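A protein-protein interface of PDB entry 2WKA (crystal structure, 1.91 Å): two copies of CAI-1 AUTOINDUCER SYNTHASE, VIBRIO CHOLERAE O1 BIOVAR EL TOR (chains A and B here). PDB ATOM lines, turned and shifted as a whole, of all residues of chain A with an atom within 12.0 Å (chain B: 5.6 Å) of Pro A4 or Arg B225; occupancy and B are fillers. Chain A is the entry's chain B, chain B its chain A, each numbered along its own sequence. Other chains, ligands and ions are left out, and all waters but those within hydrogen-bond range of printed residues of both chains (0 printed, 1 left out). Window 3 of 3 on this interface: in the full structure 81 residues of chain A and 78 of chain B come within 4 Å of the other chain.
A ring nitrogen (NE2) of His B228 sits at hydrogen-bond distance from the backbone carbonyl oxygen of Gln A5 (2.8 Å).
The backbone carbonyl oxygen of Val B227 lies within hydrogen-bond range of the side-chain amide nitrogen of Asn B248, at 3.0 Å. O of His B228 lies within hydrogen-bond range of N of Asn B248, 3.1 Å away. The backbone carbonyl oxygen (O) of His B228 is in hydrogen-bond range of the side-chain amide nitrogen (ND2) of Asn B249.
Among the printed residues, merely in contact across the chains: Pro A4 with Arg B225 (3.5 Å), Pro A4 with Glu B226 (3.7 Å), Pro A4 with Val B227 (3.6 Å), Pro A4 with His B228 (3.4 Å), Leu A6 with His B228 (3.6 Å), Leu A6 with Asn B249 (3.1 Å) and Pro A7 with His B228 (3.9 Å).
Of chain B, only Arg B225 (3.5 Å), Glu B226 (3.7 Å), Val B227 (3.6 Å) and His B228 (3.4 Å) come within 4 Å of Pro A4. Printed residues of chain B within 4 Å of Gln A5: His B228. Of the printed residues of chain B, Leu A6 touches His B228 and Asn B249. Of the printed residues of chain B, Pro A7 touches His B228. No residue of chain A comes within 4 Å of Gly B222. Arg B225 touches just one residue of chain A: Pro A4 (3.5 Å). Val B227 touches just one residue of chain A: Pro A4 (3.6 Å). Of the printed residues of chain A, His B228 touches Pro A4 (3.4 Å), Gln A5 (2.8 Å), Leu A6 (3.6 Å) and Pro A7 (3.9 Å). Of the printed residues of chain A, Asn B249 touches Leu A6. The nearest residue of chain B that does not touch Pro A4 is Asn B248 (4.1 Å). The nearest residue of chain A that does not touch Arg B225 is Gln A5 (6.9 Å).
Hydrophobic or aromatic side chains of chain B that line the printed part of chain A: His B228. Of the 11 printed residues of chain A, 4 touch a printed residue of chain B. Printed residues of chain A that touch a printed residue of chain B: Pro A4, Gln A5, Leu A6 and Pro A7. Hydrophobic or aromatic side chains of chain A within 4 Å of the printed part of chain B: Pro A4, Leu A6 and Pro A7. Among the printed residues, 8 pairs touch across the chains. Among the printed residues, no Asp or Glu carboxylate lies within 4 Å of a Lys or Arg side-chain nitrogen of the other chain.
No position is printed for both chains. Of the 8 pairs that touch across the chains among the printed residues, none has its exchanged pair printed and touching as well.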
ATOM      1  N   PRO A   4       1.524 -21.426 -23.197  1.00  0.00           N
ATOM      2  CA  PRO A   4       0.474 -22.423 -23.025  1.00  0.00           C
ATOM      3  C   PRO A   4       0.984 -23.821 -23.366  1.00  0.00           C
ATOM      4  O   PRO A   4       1.829 -23.969 -24.245  1.00  0.00           O
ATOM      5  CB  PRO A   4      -0.565 -21.986 -24.054  1.00  0.00           C
ATOM      6  CG  PRO A   4       0.267 -21.400 -25.185  1.00  0.00           C
ATOM      7  CD  PRO A   4       1.576 -20.916 -24.581  1.00  0.00           C
ATOM      8  N   GLN A   5       0.482 -24.841 -22.684  1.00  0.00           N
ATOM      9  CA  GLN A   5       0.886 -26.212 -22.990  1.00  0.00           C
ATOM     10  C   GLN A   5       0.376 -26.590 -24.376  1.00  0.00           C
ATOM     11  O   GLN A   5      -0.685 -26.125 -24.796  1.00  0.00           O
ATOM     12  CB  GLN A   5       0.333 -27.179 -21.935  1.00  0.00           C
ATOM     13  N   LEU A   6       1.130 -27.425 -25.084  1.00  0.00           N
ATOM     14  CA  LEU A   6       0.686 -27.936 -26.381  1.00  0.00           C
ATOM     15  C   LEU A   6      -0.521 -28.849 -26.213  1.00  0.00           C
ATOM     16  O   LEU A   6      -0.572 -29.629 -25.266  1.00  0.00           O
ATOM     17  CB  LEU A   6       1.786 -28.760 -27.048  1.00  0.00           C
ATOM     18  CG  LEU A   6       2.950 -28.108 -27.801  1.00  0.00           C
ATOM     19  CD1 LEU A   6       2.509 -26.822 -28.498  1.00  0.00           C
ATOM     20  CD2 LEU A   6       4.096 -27.857 -26.859  1.00  0.00           C
ATOM     21  N   PRO A   7      -1.475 -28.781 -27.157  1.00  0.00           N
ATOM     22  CA  PRO A   7      -2.545 -29.780 -27.213  1.00  0.00           C
ATOM     23  C   PRO A   7      -1.965 -31.168 -27.485  1.00  0.00           C
ATOM     24  O   PRO A   7      -0.920 -31.287 -28.128  1.00  0.00           O
ATOM     25  CB  PRO A   7      -3.415 -29.309 -28.389  1.00  0.00           C
ATOM     26  CG  PRO A   7      -2.514 -28.410 -29.216  1.00  0.00           C
ATOM     27  CD  PRO A   7      -1.556 -27.788 -28.247  1.00  0.00           C
ATOM     28  N   ASP A   8      -2.627 -32.209 -26.979  1.00  0.00           N
ATOM     29  CA  ASP A   8      -2.140 -33.580 -27.111  1.00  0.00           C
ATOM     30  C   ASP A   8      -1.732 -33.940 -28.536  1.00  0.00           C
ATOM     31  O   ASP A   8      -0.763 -34.670 -28.736  1.00  0.00           O
ATOM     32  CB  ASP A   8      -3.189 -34.592 -26.628  1.00  0.00           C
ATOM     33  CG  ASP A   8      -3.575 -34.398 -25.174  1.00  0.00           C
ATOM     34  OD1 ASP A   8      -2.764 -33.848 -24.396  1.00  0.00           O
ATOM     35  OD2 ASP A   8      -4.706 -34.799 -24.810  1.00  0.00           O
ATOM     36  N   PHE A   9      -2.478 -33.455 -29.525  1.00  0.00           N
ATOM     37  CA  PHE A   9      -2.211 -33.866 -30.907  1.00  0.00           C
ATOM     38  C   PHE A   9      -0.852 -33.375 -31.423  1.00  0.00           C
ATOM     39  O   PHE A   9      -0.250 -33.983 -32.319  1.00  0.00           O
ATOM     40  CB  PHE A   9      -3.353 -33.467 -31.850  1.00  0.00           C
ATOM     41  CG  PHE A   9      -3.353 -32.011 -32.246  1.00  0.00           C
ATOM     42  CD1 PHE A   9      -4.118 -31.095 -31.555  1.00  0.00           C
ATOM     43  CD2 PHE A   9      -2.611 -31.574 -33.332  1.00  0.00           C
ATOM     44  CE1 PHE A   9      -4.134 -29.758 -31.922  1.00  0.00           C
ATOM     45  CE2 PHE A   9      -2.627 -30.246 -33.707  1.00  0.00           C
ATOM     46  CZ  PHE A   9      -3.389 -29.338 -33.001  1.00  0.00           C
ATOM     47  N   ILE A  10      -0.344 -32.301 -30.833  1.00  0.00           N
ATOM     48  CA  ILE A  10       1.032 -31.922 -31.101  1.00  0.00           C
ATOM     49  C   ILE A  10       1.984 -32.537 -30.069  1.00  0.00           C
ATOM     50  O   ILE A  10       3.017 -33.111 -30.425  1.00  0.00           O
ATOM     51  CB  ILE A  10       1.220 -30.392 -31.140  1.00  0.00           C
ATOM     52  CG1 ILE A  10       0.272 -29.760 -32.165  1.00  0.00           C
ATOM     53  CG2 ILE A  10       2.691 -30.058 -31.451  1.00  0.00           C
ATOM     54  CD1 ILE A  10       0.216 -28.235 -32.119  1.00  0.00           C
ATOM     55  N   GLN A  11       1.631 -32.427 -28.790  1.00  0.00           N
ATOM     56  CA  GLN A  11       2.519 -32.900 -27.724  1.00  0.00           C
ATOM     57  C   GLN A  11       2.883 -34.374 -27.890  1.00  0.00           C
ATOM     58  O   GLN A  11       4.039 -34.744 -27.733  1.00  0.00           O
ATOM     59  CB  GLN A  11       1.904 -32.664 -26.341  1.00  0.00           C
ATOM     60  CG  GLN A  11       2.863 -32.958 -25.188  1.00  0.00           C
ATOM     61  CD  GLN A  11       3.993 -31.966 -25.119  1.00  0.00           C
ATOM     62  OE1 GLN A  11       3.784 -30.794 -24.794  1.00  0.00           O
ATOM     63  NE2 GLN A  11       5.206 -32.426 -25.404  1.00  0.00           N
ATOM     64  N   ASN A  12       1.897 -35.216 -28.186  1.00  0.00           N
ATOM     65  CA  ASN A  12       2.169 -36.636 -28.402  1.00  0.00           C
ATOM     66  C   ASN A  12       3.201 -36.876 -29.488  1.00  0.00           C
ATOM     67  O   ASN A  12       4.122 -37.681 -29.314  1.00  0.00           O
ATOM     68  CB  ASN A  12       0.887 -37.390 -28.749  1.00  0.00           C
ATOM     69  CG  ASN A  12      -0.027 -37.549 -27.554  1.00  0.00           C
ATOM     70  OD1 ASN A  12       0.390 -37.340 -26.411  1.00  0.00           O
ATOM     71  ND2 ASN A  12      -1.282 -37.902 -27.808  1.00  0.00           N
ATOM     72  N   ILE A  14       5.508 -34.781 -30.731  1.00  0.00           N
ATOM     73  CA  ILE A  14       6.813 -34.282 -30.315  1.00  0.00           C
ATOM     74  C   ILE A  14       7.468 -35.234 -29.303  1.00  0.00           C
ATOM     75  O   ILE A  14       8.649 -35.552 -29.421  1.00  0.00           O
ATOM     76  CB  ILE A  14       6.710 -32.858 -29.724  1.00  0.00           C
ATOM     77  CG1 ILE A  14       6.163 -31.876 -30.773  1.00  0.00           C
ATOM     78  CG2 ILE A  14       8.058 -32.408 -29.181  1.00  0.00           C
ATOM     79  CD1 ILE A  14       6.934 -31.882 -32.107  1.00  0.00           C
ATOM     80  N   ASP A  15       6.687 -35.697 -28.324  1.00  0.00           N
ATOM     81  CA  ASP A  15       7.191 -36.606 -27.288  1.00  0.00           C
ATOM     82  C   ASP A  15       7.799 -37.862 -27.887  1.00  0.00           C
ATOM     83  O   ASP A  15       8.903 -38.261 -27.528  1.00  0.00           O
ATOM     84  CB  ASP A  15       6.064 -37.021 -26.332  1.00  0.00           C
ATOM     85  CG  ASP A  15       5.739 -35.957 -25.319  1.00  0.00           C
ATOM     86  OD1 ASP A  15       6.438 -34.927 -25.285  1.00  0.00           O
ATOM     87  OD2 ASP A  15       4.777 -36.152 -24.543  1.00  0.00           O
ATOM     88  N   GLY B  98       9.550 -12.138 -26.351  1.00  0.00           N
ATOM     89  CA  GLY B  98       8.972 -12.712 -25.147  1.00  0.00           C
ATOM     90  C   GLY B  98       8.670 -14.194 -25.285  1.00  0.00           C
ATOM     91  O   GLY B  98       8.183 -14.815 -24.345  1.00  0.00           O
ATOM     92  N   GLY B 222      -0.351  -7.847 -25.106  1.00  0.00           N
ATOM     93  CA  GLY B 222      -0.074  -8.655 -23.926  1.00  0.00           C
ATOM     94  C   GLY B 222      -0.474 -10.111 -24.058  1.00  0.00           C
ATOM     95  O   GLY B 222      -0.802 -10.754 -23.069  1.00  0.00           O
ATOM     96  N   LEU B 223      -0.442 -10.647 -25.274  1.00  0.00           N
ATOM     97  CA  LEU B 223      -0.890 -12.020 -25.485  1.00  0.00           C
ATOM     98  C   LEU B 223       0.249 -13.030 -25.563  1.00  0.00           C
ATOM     99  O   LEU B 223       0.023 -14.240 -25.597  1.00  0.00           O
ATOM    100  CB  LEU B 223      -1.757 -12.108 -26.743  1.00  0.00           C
ATOM    101  CG  LEU B 223      -3.033 -11.266 -26.722  1.00  0.00           C
ATOM    102  CD1 LEU B 223      -3.600 -11.111 -28.135  1.00  0.00           C
ATOM    103  CD2 LEU B 223      -4.073 -11.863 -25.757  1.00  0.00           C
ATOM    104  N   THR B 224       1.478 -12.528 -25.587  1.00  0.00           N
ATOM    105  CA  THR B 224       2.648 -13.369 -25.818  1.00  0.00           C
ATOM    106  C   THR B 224       2.621 -14.733 -25.141  1.00  0.00           C
ATOM    107  O   THR B 224       2.812 -15.757 -25.802  1.00  0.00           O
ATOM    108  CB  THR B 224       3.940 -12.658 -25.408  1.00  0.00           C
ATOM    109  OG1 THR B 224       4.018 -11.413 -26.093  1.00  0.00           O
ATOM    110  CG2 THR B 224       5.140 -13.509 -25.779  1.00  0.00           C
ATOM    111  N   ARG B 225       2.413 -14.743 -23.827  1.00  0.00           N
ATOM    112  CA  ARG B 225       2.424 -15.980 -23.050  1.00  0.00           C
ATOM    113  C   ARG B 225       1.210 -16.872 -23.316  1.00  0.00           C
ATOM    114  O   ARG B 225       1.103 -17.954 -22.753  1.00  0.00           O
ATOM    115  CB  ARG B 225       2.488 -15.679 -21.546  1.00  0.00           C
ATOM    116  CG  ARG B 225       3.793 -15.063 -21.079  1.00  0.00           C
ATOM    117  CD  ARG B 225       4.878 -16.114 -20.855  1.00  0.00           C
ATOM    118  NE  ARG B 225       4.611 -16.922 -19.665  1.00  0.00           N
ATOM    119  CZ  ARG B 225       4.734 -16.475 -18.418  1.00  0.00           C
ATOM    120  NH1 ARG B 225       5.123 -15.222 -18.198  1.00  0.00           N
ATOM    121  NH2 ARG B 225       4.470 -17.274 -17.389  1.00  0.00           N
ATOM    122  N   GLU B 226       0.292 -16.424 -24.160  1.00  0.00           N
ATOM    123  CA  GLU B 226      -0.872 -17.240 -24.444  1.00  0.00           C
ATOM    124  C   GLU B 226      -0.868 -17.823 -25.854  1.00  0.00           C
ATOM    125  O   GLU B 226      -1.811 -18.502 -26.247  1.00  0.00           O
ATOM    126  CB  GLU B 226      -2.154 -16.444 -24.185  1.00  0.00           C
ATOM    127  CG  GLU B 226      -2.544 -16.416 -22.710  1.00  0.00           C
ATOM    128  CD  GLU B 226      -4.032 -16.224 -22.512  1.00  0.00           C
ATOM    129  OE1 GLU B 226      -4.727 -17.233 -22.254  1.00  0.00           O
ATOM    130  OE2 GLU B 226      -4.512 -15.074 -22.634  1.00  0.00           O
ATOM    131  N   VAL B 227       0.195 -17.562 -26.605  1.00  0.00           N
ATOM    132  CA  VAL B 227       0.300 -18.069 -27.971  1.00  0.00           C
ATOM    133  C   VAL B 227       1.374 -19.152 -28.071  1.00  0.00           C
ATOM    134  O   VAL B 227       2.473 -19.009 -27.520  1.00  0.00           O
ATOM    135  CB  VAL B 227       0.601 -16.922 -28.964  1.00  0.00           C
ATOM    136  CG1 VAL B 227       0.737 -17.457 -30.385  1.00  0.00           C
ATOM    137  CG2 VAL B 227      -0.479 -15.860 -28.884  1.00  0.00           C
ATOM    138  N   HIS B 228       1.056 -20.242 -28.761  1.00  0.00           N
ATOM    139  CA  HIS B 228       2.009 -21.333 -28.925  1.00  0.00           C
ATOM    140  C   HIS B 228       3.171 -21.010 -29.878  1.00  0.00           C
ATOM    141  O   HIS B 228       4.324 -21.343 -29.595  1.00  0.00           O
ATOM    142  CB  HIS B 228       1.296 -22.598 -29.404  1.00  0.00           C
ATOM    143  CG  HIS B 228       0.293 -23.127 -28.426  1.00  0.00           C
ATOM    144  ND1 HIS B 228      -0.981 -22.615 -28.318  1.00  0.00           N
ATOM    145  CD2 HIS B 228       0.379 -24.119 -27.509  1.00  0.00           C
ATOM    146  CE1 HIS B 228      -1.637 -23.265 -27.374  1.00  0.00           C
ATOM    147  NE2 HIS B 228      -0.835 -24.185 -26.870  1.00  0.00           N
ATOM    148  N   ASN B 248       6.754 -21.200 -27.728  1.00  0.00           N
ATOM    149  CA  ASN B 248       6.628 -21.198 -26.276  1.00  0.00           C
ATOM    150  C   ASN B 248       6.542 -22.620 -25.745  1.00  0.00           C
ATOM    151  O   ASN B 248       5.744 -22.928 -24.867  1.00  0.00           O
ATOM    152  CB  ASN B 248       5.430 -20.355 -25.831  1.00  0.00           C
ATOM    153  CG  ASN B 248       5.780 -18.887 -25.705  1.00  0.00           C
ATOM    154  OD1 ASN B 248       6.928 -18.544 -25.449  1.00  0.00           O
ATOM    155  ND2 ASN B 248       4.795 -18.013 -25.894  1.00  0.00           N
ATOM    156  N   ASN B 249       7.401 -23.473 -26.292  1.00  0.00           N
ATOM    157  CA  ASN B 249       7.402 -24.895 -26.046  1.00  0.00           C
ATOM    158  C   ASN B 249       8.686 -25.431 -26.679  1.00  0.00           C
ATOM    159  O   ASN B 249       9.567 -24.647 -27.047  1.00  0.00           O
ATOM    160  CB  ASN B 249       6.169 -25.529 -26.687  1.00  0.00           C
ATOM    161  CG  ASN B 249       5.989 -25.097 -28.134  1.00  0.00           C
ATOM    162  OD1 ASN B 249       6.770 -25.474 -28.999  1.00  0.00           O
ATOM    163  ND2 ASN B 249       4.953 -24.306 -28.398  1.00  0.00           N
